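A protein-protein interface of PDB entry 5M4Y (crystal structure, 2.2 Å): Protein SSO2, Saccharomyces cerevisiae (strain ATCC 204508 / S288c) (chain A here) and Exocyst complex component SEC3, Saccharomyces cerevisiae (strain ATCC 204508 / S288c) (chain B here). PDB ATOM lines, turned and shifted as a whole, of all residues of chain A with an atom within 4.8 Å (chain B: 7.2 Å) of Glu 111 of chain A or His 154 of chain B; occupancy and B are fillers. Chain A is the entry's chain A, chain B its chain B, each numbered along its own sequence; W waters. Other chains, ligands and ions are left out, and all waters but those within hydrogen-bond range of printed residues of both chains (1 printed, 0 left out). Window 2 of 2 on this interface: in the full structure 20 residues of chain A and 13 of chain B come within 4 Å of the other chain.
The side-chain hydroxyl (OG) of Ser 107 of chain A sits at hydrogen-bond distance from the backbone carbonyl oxygen (O) of Glu 152 of chain B.
NE of Arg 175 of chain B lies within hydrogen-bond range of OD1 of Asn 108 of chain A (2.8 Å).
OE1 of Glu 152 of chain B is in salt-bridge range of NZ of Lys 110 of chain A.
The side-chain carboxylate of Glu 111 of chain A sits at hydrogen-bond distance from a ring nitrogen (NE2) of His 154 of chain B.
Of the 17 printed residues of chain B, 3 touch a printed residue of chain A.
Printed residues of chain B that touch a printed residue of chain A: Glu 152, His 154 and Arg 175.
Hydrophobic or aromatic side chains of chain B that line the printed part of chain A: His 154.
Printed residues of chain A that touch a printed residue of chain B: Ser 107, Asn 108, Lys 110 and Glu 111.
Among the printed residues, Asp or Glu carboxylates within 4 Å of a Lys or Arg side-chain nitrogen of the other chain: Lys 110 of chain A with Glu 152 of chain B (2.6 Å).
The backbone carbonyl oxygen (O) of Phe 151 of chain B is in hydrogen-bond range of a ring nitrogen (ND1) of His 154 of chain B, 2.6 Å away.
A ring nitrogen (ND1) of His 154 of chain B sits at hydrogen-bond distance from the backbone carbonyl oxygen (O) of Glu 152 of chain B.
CE1 of His 154 of chain B touches OG of Ser 107 of chain A, 3.8 Å away.
Printed residues of chain B within 4 Å of Ser 107 of chain A: Glu 152 and His 154.
Of the printed residues of chain B, Lys 110 of chain A touches Glu 152.
Thr 150 of chain B touches none of the printed residues of chain A.
His 154 of chain B touches two residues of chain A.
Ala 176 of chain B touches none of the printed residues of chain A.
The nearest residue of chain B that does not touch Glu 111 of chain A is Glu 152 of chain B (5.9 Å).
Water W1 lies within hydrogen-bond range of ND2 of Asn 108 of chain A, OE2 of Glu 111 of chain A, OG of Ser 107 of chain A and NE2 of His 154 of chain B.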
ATOM      1  N   SER A 107      24.330 -28.227 -31.881  1.00  0.00           N
ATOM      2  CA  SER A 107      23.719 -28.239 -30.557  1.00  0.00           C
ATOM      3  C   SER A 107      22.955 -26.948 -30.294  1.00  0.00           C
ATOM      4  O   SER A 107      21.826 -26.973 -29.789  1.00  0.00           O
ATOM      5  CB  SER A 107      24.791 -28.454 -29.491  1.00  0.00           C
ATOM      6  OG  SER A 107      24.255 -28.285 -28.192  1.00  0.00           O
ATOM      7  N   ASN A 108      23.564 -25.805 -30.622  1.00  0.00           N
ATOM      8  CA  ASN A 108      22.882 -24.525 -30.459  1.00  0.00           C
ATOM      9  C   ASN A 108      21.609 -24.472 -31.291  1.00  0.00           C
ATOM     10  O   ASN A 108      20.558 -24.031 -30.814  1.00  0.00           O
ATOM     11  CB  ASN A 108      23.814 -23.375 -30.843  1.00  0.00           C
ATOM     12  CG  ASN A 108      24.942 -23.180 -29.853  1.00  0.00           C
ATOM     13  OD1 ASN A 108      25.938 -22.521 -30.150  1.00  0.00           O
ATOM     14  ND2 ASN A 108      24.793 -23.759 -28.669  1.00  0.00           N
ATOM     15  N   TYR A 109      21.686 -24.929 -32.541  1.00  0.00           N
ATOM     16  CA  TYR A 109      20.523 -24.886 -33.420  1.00  0.00           C
ATOM     17  C   TYR A 109      19.409 -25.787 -32.909  1.00  0.00           C
ATOM     18  O   TYR A 109      18.227 -25.459 -33.053  1.00  0.00           O
ATOM     19  CB  TYR A 109      20.932 -25.278 -34.837  1.00  0.00           C
ATOM     20  CG  TYR A 109      19.806 -25.245 -35.845  1.00  0.00           C
ATOM     21  CD1 TYR A 109      19.069 -24.086 -36.054  1.00  0.00           C
ATOM     22  CD2 TYR A 109      19.488 -26.366 -36.599  1.00  0.00           C
ATOM     23  CE1 TYR A 109      18.044 -24.049 -36.977  1.00  0.00           C
ATOM     24  CE2 TYR A 109      18.466 -26.339 -37.523  1.00  0.00           C
ATOM     25  CZ  TYR A 109      17.748 -25.177 -37.708  1.00  0.00           C
ATOM     26  OH  TYR A 109      16.727 -25.140 -38.628  1.00  0.00           O
ATOM     27  N   LYS A 110      19.765 -26.922 -32.304  1.00  0.00           N
ATOM     28  CA  LYS A 110      18.754 -27.821 -31.756  1.00  0.00           C
ATOM     29  C   LYS A 110      17.992 -27.163 -30.612  1.00  0.00           C
ATOM     30  O   LYS A 110      16.763 -27.272 -30.536  1.00  0.00           O
ATOM     31  CB  LYS A 110      19.410 -29.119 -31.291  1.00  0.00           C
ATOM     32  CG  LYS A 110      18.441 -30.122 -30.688  1.00  0.00           C
ATOM     33  CD  LYS A 110      19.161 -31.365 -30.201  1.00  0.00           C
ATOM     34  CE  LYS A 110      18.198 -32.322 -29.523  1.00  0.00           C
ATOM     35  NZ  LYS A 110      18.900 -33.505 -28.956  1.00  0.00           N
ATOM     36  N   GLU A 111      18.704 -26.483 -29.710  1.00  0.00           N
ATOM     37  CA  GLU A 111      18.040 -25.789 -28.610  1.00  0.00           C
ATOM     38  C   GLU A 111      17.111 -24.701 -29.130  1.00  0.00           C
ATOM     39  O   GLU A 111      15.921 -24.671 -28.796  1.00  0.00           O
ATOM     40  CB  GLU A 111      19.076 -25.186 -27.665  1.00  0.00           C
ATOM     41  CG  GLU A 111      19.859 -26.179 -26.839  1.00  0.00           C
ATOM     42  CD  GLU A 111      20.845 -25.490 -25.921  1.00  0.00           C
ATOM     43  OE1 GLU A 111      20.933 -24.246 -25.974  1.00  0.00           O
ATOM     44  OE2 GLU A 111      21.532 -26.187 -25.149  1.00  0.00           O
ATOM     45  N   GLU A 112      17.646 -23.793 -29.949  1.00  0.00           N
ATOM     46  CA  GLU A 112      16.845 -22.686 -30.457  1.00  0.00           C
ATOM     47  C   GLU A 112      15.696 -23.173 -31.330  1.00  0.00           C
ATOM     48  O   GLU A 112      14.664 -22.501 -31.428  1.00  0.00           O
ATOM     49  CB  GLU A 112      17.738 -21.710 -31.223  1.00  0.00           C
ATOM     50  CG  GLU A 112      18.771 -21.016 -30.344  1.00  0.00           C
ATOM     51  CD  GLU A 112      19.792 -20.224 -31.139  1.00  0.00           C
ATOM     52  OE1 GLU A 112      19.795 -20.333 -32.383  1.00  0.00           O
ATOM     53  OE2 GLU A 112      20.593 -19.494 -30.521  1.00  0.00           O
ATOM     54  N   SER A 113      15.848 -24.338 -31.966  1.00  0.00           N
ATOM     55  CA  SER A 113      14.729 -24.915 -32.704  1.00  0.00           C
ATOM     56  C   SER A 113      13.696 -25.519 -31.763  1.00  0.00           C
ATOM     57  O   SER A 113      12.498 -25.504 -32.068  1.00  0.00           O
ATOM     58  CB  SER A 113      15.234 -25.967 -33.692  1.00  0.00           C
ATOM     59  OG  SER A 113      14.214 -26.354 -34.596  1.00  0.00           O
ATOM     60  N   LYS A 114      14.137 -26.056 -30.622  1.00  0.00           N
ATOM     61  CA  LYS A 114      13.196 -26.526 -29.610  1.00  0.00           C
ATOM     62  C   LYS A 114      12.439 -25.360 -28.990  1.00  0.00           C
ATOM     63  O   LYS A 114      11.215 -25.421 -28.822  1.00  0.00           O
ATOM     64  CB  LYS A 114      13.935 -27.321 -28.532  1.00  0.00           C
ATOM     65  CG  LYS A 114      14.199 -28.777 -28.882  1.00  0.00           C
ATOM     66  CD  LYS A 114      15.011 -29.456 -27.790  1.00  0.00           C
ATOM     67  CE  LYS A 114      15.139 -30.953 -28.026  1.00  0.00           C
ATOM     68  NZ  LYS A 114      13.841 -31.658 -27.845  1.00  0.00           N
ATOM     69  N   GLU A 115      13.155 -24.288 -28.638  1.00  0.00           N
ATOM     70  CA  GLU A 115      12.506 -23.113 -28.068  1.00  0.00           C
ATOM     71  C   GLU A 115      11.501 -22.502 -29.036  1.00  0.00           C
ATOM     72  O   GLU A 115      10.464 -21.984 -28.606  1.00  0.00           O
ATOM     73  CB  GLU A 115      13.555 -22.076 -27.668  1.00  0.00           C
ATOM     74  CG  GLU A 115      14.353 -22.444 -26.427  1.00  0.00           C
ATOM     75  CD  GLU A 115      13.534 -22.337 -25.156  1.00  0.00           C
ATOM     76  OE1 GLU A 115      12.520 -21.606 -25.161  1.00  0.00           O
ATOM     77  OE2 GLU A 115      13.900 -22.984 -24.154  1.00  0.00           O
ATOM     78  N   ILE B 144      35.983 -34.663 -19.708  1.00  0.00           N
ATOM     79  CA  ILE B 144      35.333 -33.576 -20.432  1.00  0.00           C
ATOM     80  C   ILE B 144      34.838 -34.056 -21.791  1.00  0.00           C
ATOM     81  O   ILE B 144      33.717 -33.735 -22.201  1.00  0.00           O
ATOM     82  CB  ILE B 144      36.286 -32.374 -20.556  1.00  0.00           C
ATOM     83  CG1 ILE B 144      36.695 -31.877 -19.168  1.00  0.00           C
ATOM     84  CG2 ILE B 144      35.634 -31.253 -21.348  1.00  0.00           C
ATOM     85  CD1 ILE B 144      35.525 -31.481 -18.290  1.00  0.00           C
ATOM     86  N   THR B 145      35.657 -34.834 -22.505  1.00  0.00           N
ATOM     87  CA  THR B 145      35.230 -35.380 -23.790  1.00  0.00           C
ATOM     88  C   THR B 145      33.950 -36.196 -23.646  1.00  0.00           C
ATOM     89  O   THR B 145      33.027 -36.069 -24.460  1.00  0.00           O
ATOM     90  CB  THR B 145      36.342 -36.236 -24.401  1.00  0.00           C
ATOM     91  OG1 THR B 145      37.446 -35.402 -24.771  1.00  0.00           O
ATOM     92  CG2 THR B 145      35.840 -36.973 -25.628  1.00  0.00           C
ATOM     93  N   LEU B 146      33.871 -37.028 -22.605  1.00  0.00           N
ATOM     94  CA  LEU B 146      32.665 -37.816 -22.379  1.00  0.00           C
ATOM     95  C   LEU B 146      31.468 -36.929 -22.060  1.00  0.00           C
ATOM     96  O   LEU B 146      30.331 -37.278 -22.399  1.00  0.00           O
ATOM     97  CB  LEU B 146      32.900 -38.823 -21.253  1.00  0.00           C
ATOM     98  CG  LEU B 146      31.808 -39.866 -21.013  1.00  0.00           C
ATOM     99  CD1 LEU B 146      31.517 -40.628 -22.294  1.00  0.00           C
ATOM    100  CD2 LEU B 146      32.203 -40.821 -19.893  1.00  0.00           C
ATOM    101  N   TYR B 147      31.700 -35.781 -21.422  1.00  0.00           N
ATOM    102  CA  TYR B 147      30.599 -34.881 -21.094  1.00  0.00           C
ATOM    103  C   TYR B 147      30.022 -34.241 -22.351  1.00  0.00           C
ATOM    104  O   TYR B 147      28.802 -34.227 -22.546  1.00  0.00           O
ATOM    105  CB  TYR B 147      31.071 -33.811 -20.109  1.00  0.00           C
ATOM    106  CG  TYR B 147      29.955 -32.986 -19.506  1.00  0.00           C
ATOM    107  CD1 TYR B 147      29.346 -31.967 -20.228  1.00  0.00           C
ATOM    108  CD2 TYR B 147      29.514 -33.222 -18.213  1.00  0.00           C
ATOM    109  CE1 TYR B 147      28.328 -31.211 -19.682  1.00  0.00           C
ATOM    110  CE2 TYR B 147      28.498 -32.471 -17.656  1.00  0.00           C
ATOM    111  CZ  TYR B 147      27.908 -31.466 -18.396  1.00  0.00           C
ATOM    112  OH  TYR B 147      26.895 -30.715 -17.849  1.00  0.00           O
ATOM    113  N   ILE B 148      30.887 -33.693 -23.210  1.00  0.00           N
ATOM    114  CA  ILE B 148      30.426 -33.067 -24.448  1.00  0.00           C
ATOM    115  C   ILE B 148      29.651 -34.068 -25.290  1.00  0.00           C
ATOM    116  O   ILE B 148      28.631 -33.732 -25.906  1.00  0.00           O
ATOM    117  CB  ILE B 148      31.616 -32.487 -25.233  1.00  0.00           C
ATOM    118  CG1 ILE B 148      32.593 -31.786 -24.291  1.00  0.00           C
ATOM    119  CG2 ILE B 148      31.129 -31.528 -26.306  1.00  0.00           C
ATOM    120  CD1 ILE B 148      33.830 -31.239 -24.975  1.00  0.00           C
ATOM    121  N   GLN B 149      30.123 -35.312 -25.328  1.00  0.00           N
ATOM    122  CA  GLN B 149      29.452 -36.346 -26.104  1.00  0.00           C
ATOM    123  C   GLN B 149      28.121 -36.737 -25.475  1.00  0.00           C
ATOM    124  O   GLN B 149      27.136 -36.969 -26.186  1.00  0.00           O
ATOM    125  CB  GLN B 149      30.372 -37.558 -26.230  1.00  0.00           C
ATOM    126  CG  GLN B 149      29.674 -38.849 -26.582  1.00  0.00           C
ATOM    127  CD  GLN B 149      30.618 -40.028 -26.561  1.00  0.00           C
ATOM    128  OE1 GLN B 149      31.777 -39.915 -26.958  1.00  0.00           O
ATOM    129  NE2 GLN B 149      30.132 -41.166 -26.083  1.00  0.00           N
ATOM    130  N   THR B 150      28.069 -36.797 -24.143  1.00  0.00           N
ATOM    131  CA  THR B 150      26.862 -37.231 -23.446  1.00  0.00           C
ATOM    132  C   THR B 150      25.760 -36.180 -23.491  1.00  0.00           C
ATOM    133  O   THR B 150      24.595 -36.512 -23.729  1.00  0.00           O
ATOM    134  CB  THR B 150      27.194 -37.584 -21.996  1.00  0.00           C
ATOM    135  OG1 THR B 150      28.130 -38.665 -21.970  1.00  0.00           O
ATOM    136  CG2 THR B 150      25.938 -37.990 -21.239  1.00  0.00           C
ATOM    137  N   PHE B 151      26.096 -34.911 -23.258  1.00  0.00           N
ATOM    138  CA  PHE B 151      25.096 -33.857 -23.155  1.00  0.00           C
ATOM    139  C   PHE B 151      25.064 -32.956 -24.387  1.00  0.00           C
ATOM    140  O   PHE B 151      24.801 -31.756 -24.277  1.00  0.00           O
ATOM    141  CB  PHE B 151      25.318 -33.038 -21.886  1.00  0.00           C
ATOM    142  CG  PHE B 151      25.175 -33.840 -20.630  1.00  0.00           C
ATOM    143  CD1 PHE B 151      23.923 -34.221 -20.176  1.00  0.00           C
ATOM    144  CD2 PHE B 151      26.291 -34.232 -19.911  1.00  0.00           C
ATOM    145  CE1 PHE B 151      23.788 -34.970 -19.022  1.00  0.00           C
ATOM    146  CE2 PHE B 151      26.163 -34.978 -18.756  1.00  0.00           C
ATOM    147  CZ  PHE B 151      24.911 -35.348 -18.311  1.00  0.00           C
ATOM    148  N   GLU B 152      25.337 -33.530 -25.558  1.00  0.00           N
ATOM    149  CA  GLU B 152      25.079 -32.904 -26.855  1.00  0.00           C
ATOM    150  C   GLU B 152      25.716 -31.517 -26.958  1.00  0.00           C
ATOM    151  O   GLU B 152      25.040 -30.497 -27.089  1.00  0.00           O
ATOM    152  CB  GLU B 152      23.574 -32.839 -27.126  1.00  0.00           C
ATOM    153  CG  GLU B 152      22.874 -34.183 -27.019  1.00  0.00           C
ATOM    154  CD  GLU B 152      21.366 -34.063 -27.095  1.00  0.00           C
ATOM    155  OE1 GLU B 152      20.866 -32.936 -27.288  1.00  0.00           O
ATOM    156  OE2 GLU B 152      20.678 -35.097 -26.958  1.00  0.00           O
ATOM    157  N   GLY B 153      27.044 -31.499 -26.901  1.00  0.00           N
ATOM    158  CA  GLY B 153      27.773 -30.267 -27.129  1.00  0.00           C
ATOM    159  C   GLY B 153      27.731 -29.275 -25.989  1.00  0.00           C
ATOM    160  O   GLY B 153      27.790 -28.066 -26.228  1.00  0.00           O
ATOM    161  N   HIS B 154      27.628 -29.752 -24.755  1.00  0.00           N
ATOM    162  CA  HIS B 154      27.708 -28.902 -23.579  1.00  0.00           C
ATOM    163  C   HIS B 154      28.936 -29.273 -22.759  1.00  0.00           C
ATOM    164  O   HIS B 154      29.437 -30.397 -22.826  1.00  0.00           O
ATOM    165  CB  HIS B 154      26.449 -29.024 -22.714  1.00  0.00           C
ATOM    166  CG  HIS B 154      25.218 -28.451 -23.346  1.00  0.00           C
ATOM    167  ND1 HIS B 154      24.364 -29.201 -24.124  1.00  0.00           N
ATOM    168  CD2 HIS B 154      24.695 -27.203 -23.309  1.00  0.00           C
ATOM    169  CE1 HIS B 154      23.368 -28.440 -24.540  1.00  0.00           C
ATOM    170  NE2 HIS B 154      23.545 -27.223 -24.060  1.00  0.00           N
ATOM    171  N   VAL B 155      29.425 -28.302 -21.990  1.00  0.00           N
ATOM    172  CA  VAL B 155      30.562 -28.528 -21.096  1.00  0.00           C
ATOM    173  C   VAL B 155      30.276 -27.883 -19.752  1.00  0.00           C
ATOM    174  O   VAL B 155      29.542 -26.895 -19.652  1.00  0.00           O
ATOM    175  CB  VAL B 155      31.880 -27.956 -21.670  1.00  0.00           C
ATOM    176  CG1 VAL B 155      32.216 -28.594 -22.996  1.00  0.00           C
ATOM    177  CG2 VAL B 155      31.794 -26.453 -21.830  1.00  0.00           C
ATOM    178  N   PRO B 156      30.843 -28.448 -18.690  1.00  0.00           N
ATOM    179  CA  PRO B 156      30.820 -27.757 -17.397  1.00  0.00           C
ATOM    180  C   PRO B 156      31.770 -26.571 -17.417  1.00  0.00           C
ATOM    181  O   PRO B 156      32.502 -26.338 -18.381  1.00  0.00           O
ATOM    182  CB  PRO B 156      31.280 -28.835 -16.413  1.00  0.00           C
ATOM    183  CG  PRO B 156      32.122 -29.748 -17.239  1.00  0.00           C
ATOM    184  CD  PRO B 156      31.487 -29.767 -18.600  1.00  0.00           C
ATOM    185  N   ARG B 175      30.056 -20.863 -26.364  1.00  0.00           N
ATOM    186  CA  ARG B 175      28.814 -21.336 -26.961  1.00  0.00           C
ATOM    187  C   ARG B 175      28.326 -22.631 -26.330  1.00  0.00           C
ATOM    188  O   ARG B 175      27.149 -22.971 -26.480  1.00  0.00           O
ATOM    189  CB  ARG B 175      28.987 -21.533 -28.469  1.00  0.00           C
ATOM    190  CG  ARG B 175      29.279 -20.255 -29.235  1.00  0.00           C
ATOM    191  CD  ARG B 175      29.243 -20.474 -30.742  1.00  0.00           C
ATOM    192  NE  ARG B 175      27.930 -20.919 -31.204  1.00  0.00           N
ATOM    193  CZ  ARG B 175      27.542 -20.906 -32.475  1.00  0.00           C
ATOM    194  NH1 ARG B 175      28.363 -20.462 -33.416  1.00  0.00           N
ATOM    195  NH2 ARG B 175      26.329 -21.331 -32.805  1.00  0.00           N
ATOM    196  N   ALA B 176      29.194 -23.357 -25.625  1.00  0.00           N
ATOM    197  CA  ALA B 176      28.858 -24.680 -25.124  1.00  0.00           C
ATOM    198  C   ALA B 176      28.712 -24.765 -23.613  1.00  0.00           C
ATOM    199  O   ALA B 176      28.050 -25.688 -23.132  1.00  0.00           O
ATOM    200  CB  ALA B 176      29.917 -25.701 -25.568  1.00  0.00           C
ATOM    201  N   VAL B 177      29.301 -23.837 -22.858  1.00  0.00           N
ATOM    202  CA  VAL B 177      29.334 -23.968 -21.406  1.00  0.00           C
ATOM    203  C   VAL B 177      27.924 -23.880 -20.834  1.00  0.00           C
ATOM    204  O   VAL B 177      27.051 -23.177 -21.360  1.00  0.00           O
ATOM    205  CB  VAL B 177      30.267 -22.908 -20.788  1.00  0.00           C
ATOM    206  CG1 VAL B 177      29.667 -21.513 -20.902  1.00  0.00           C
ATOM    207  CG2 VAL B 177      30.591 -23.254 -19.338  1.00  0.00           C
ATOM    208  N   ILE B 178      27.691 -24.627 -19.750  1.00  0.00           N
ATOM    209  CA  ILE B 178      26.376 -24.654 -19.122  1.00  0.00           C
ATOM    210  C   ILE B 178      26.061 -23.350 -18.405  1.00  0.00           C
ATOM    211  O   ILE B 178      24.898 -23.101 -18.066  1.00  0.00           O
ATOM    212  CB  ILE B 178      26.270 -25.839 -18.143  1.00  0.00           C
ATOM    213  CG1 ILE B 178      27.383 -25.766 -17.095  1.00  0.00           C
ATOM    214  CG2 ILE B 178      26.322 -27.161 -18.893  1.00  0.00           C
ATOM    215  CD1 ILE B 178      27.330 -26.878 -16.065  1.00  0.00           C
HETATM  216  O   HOH W   1      23.712 -25.624 -26.971  1.00  0.00           O
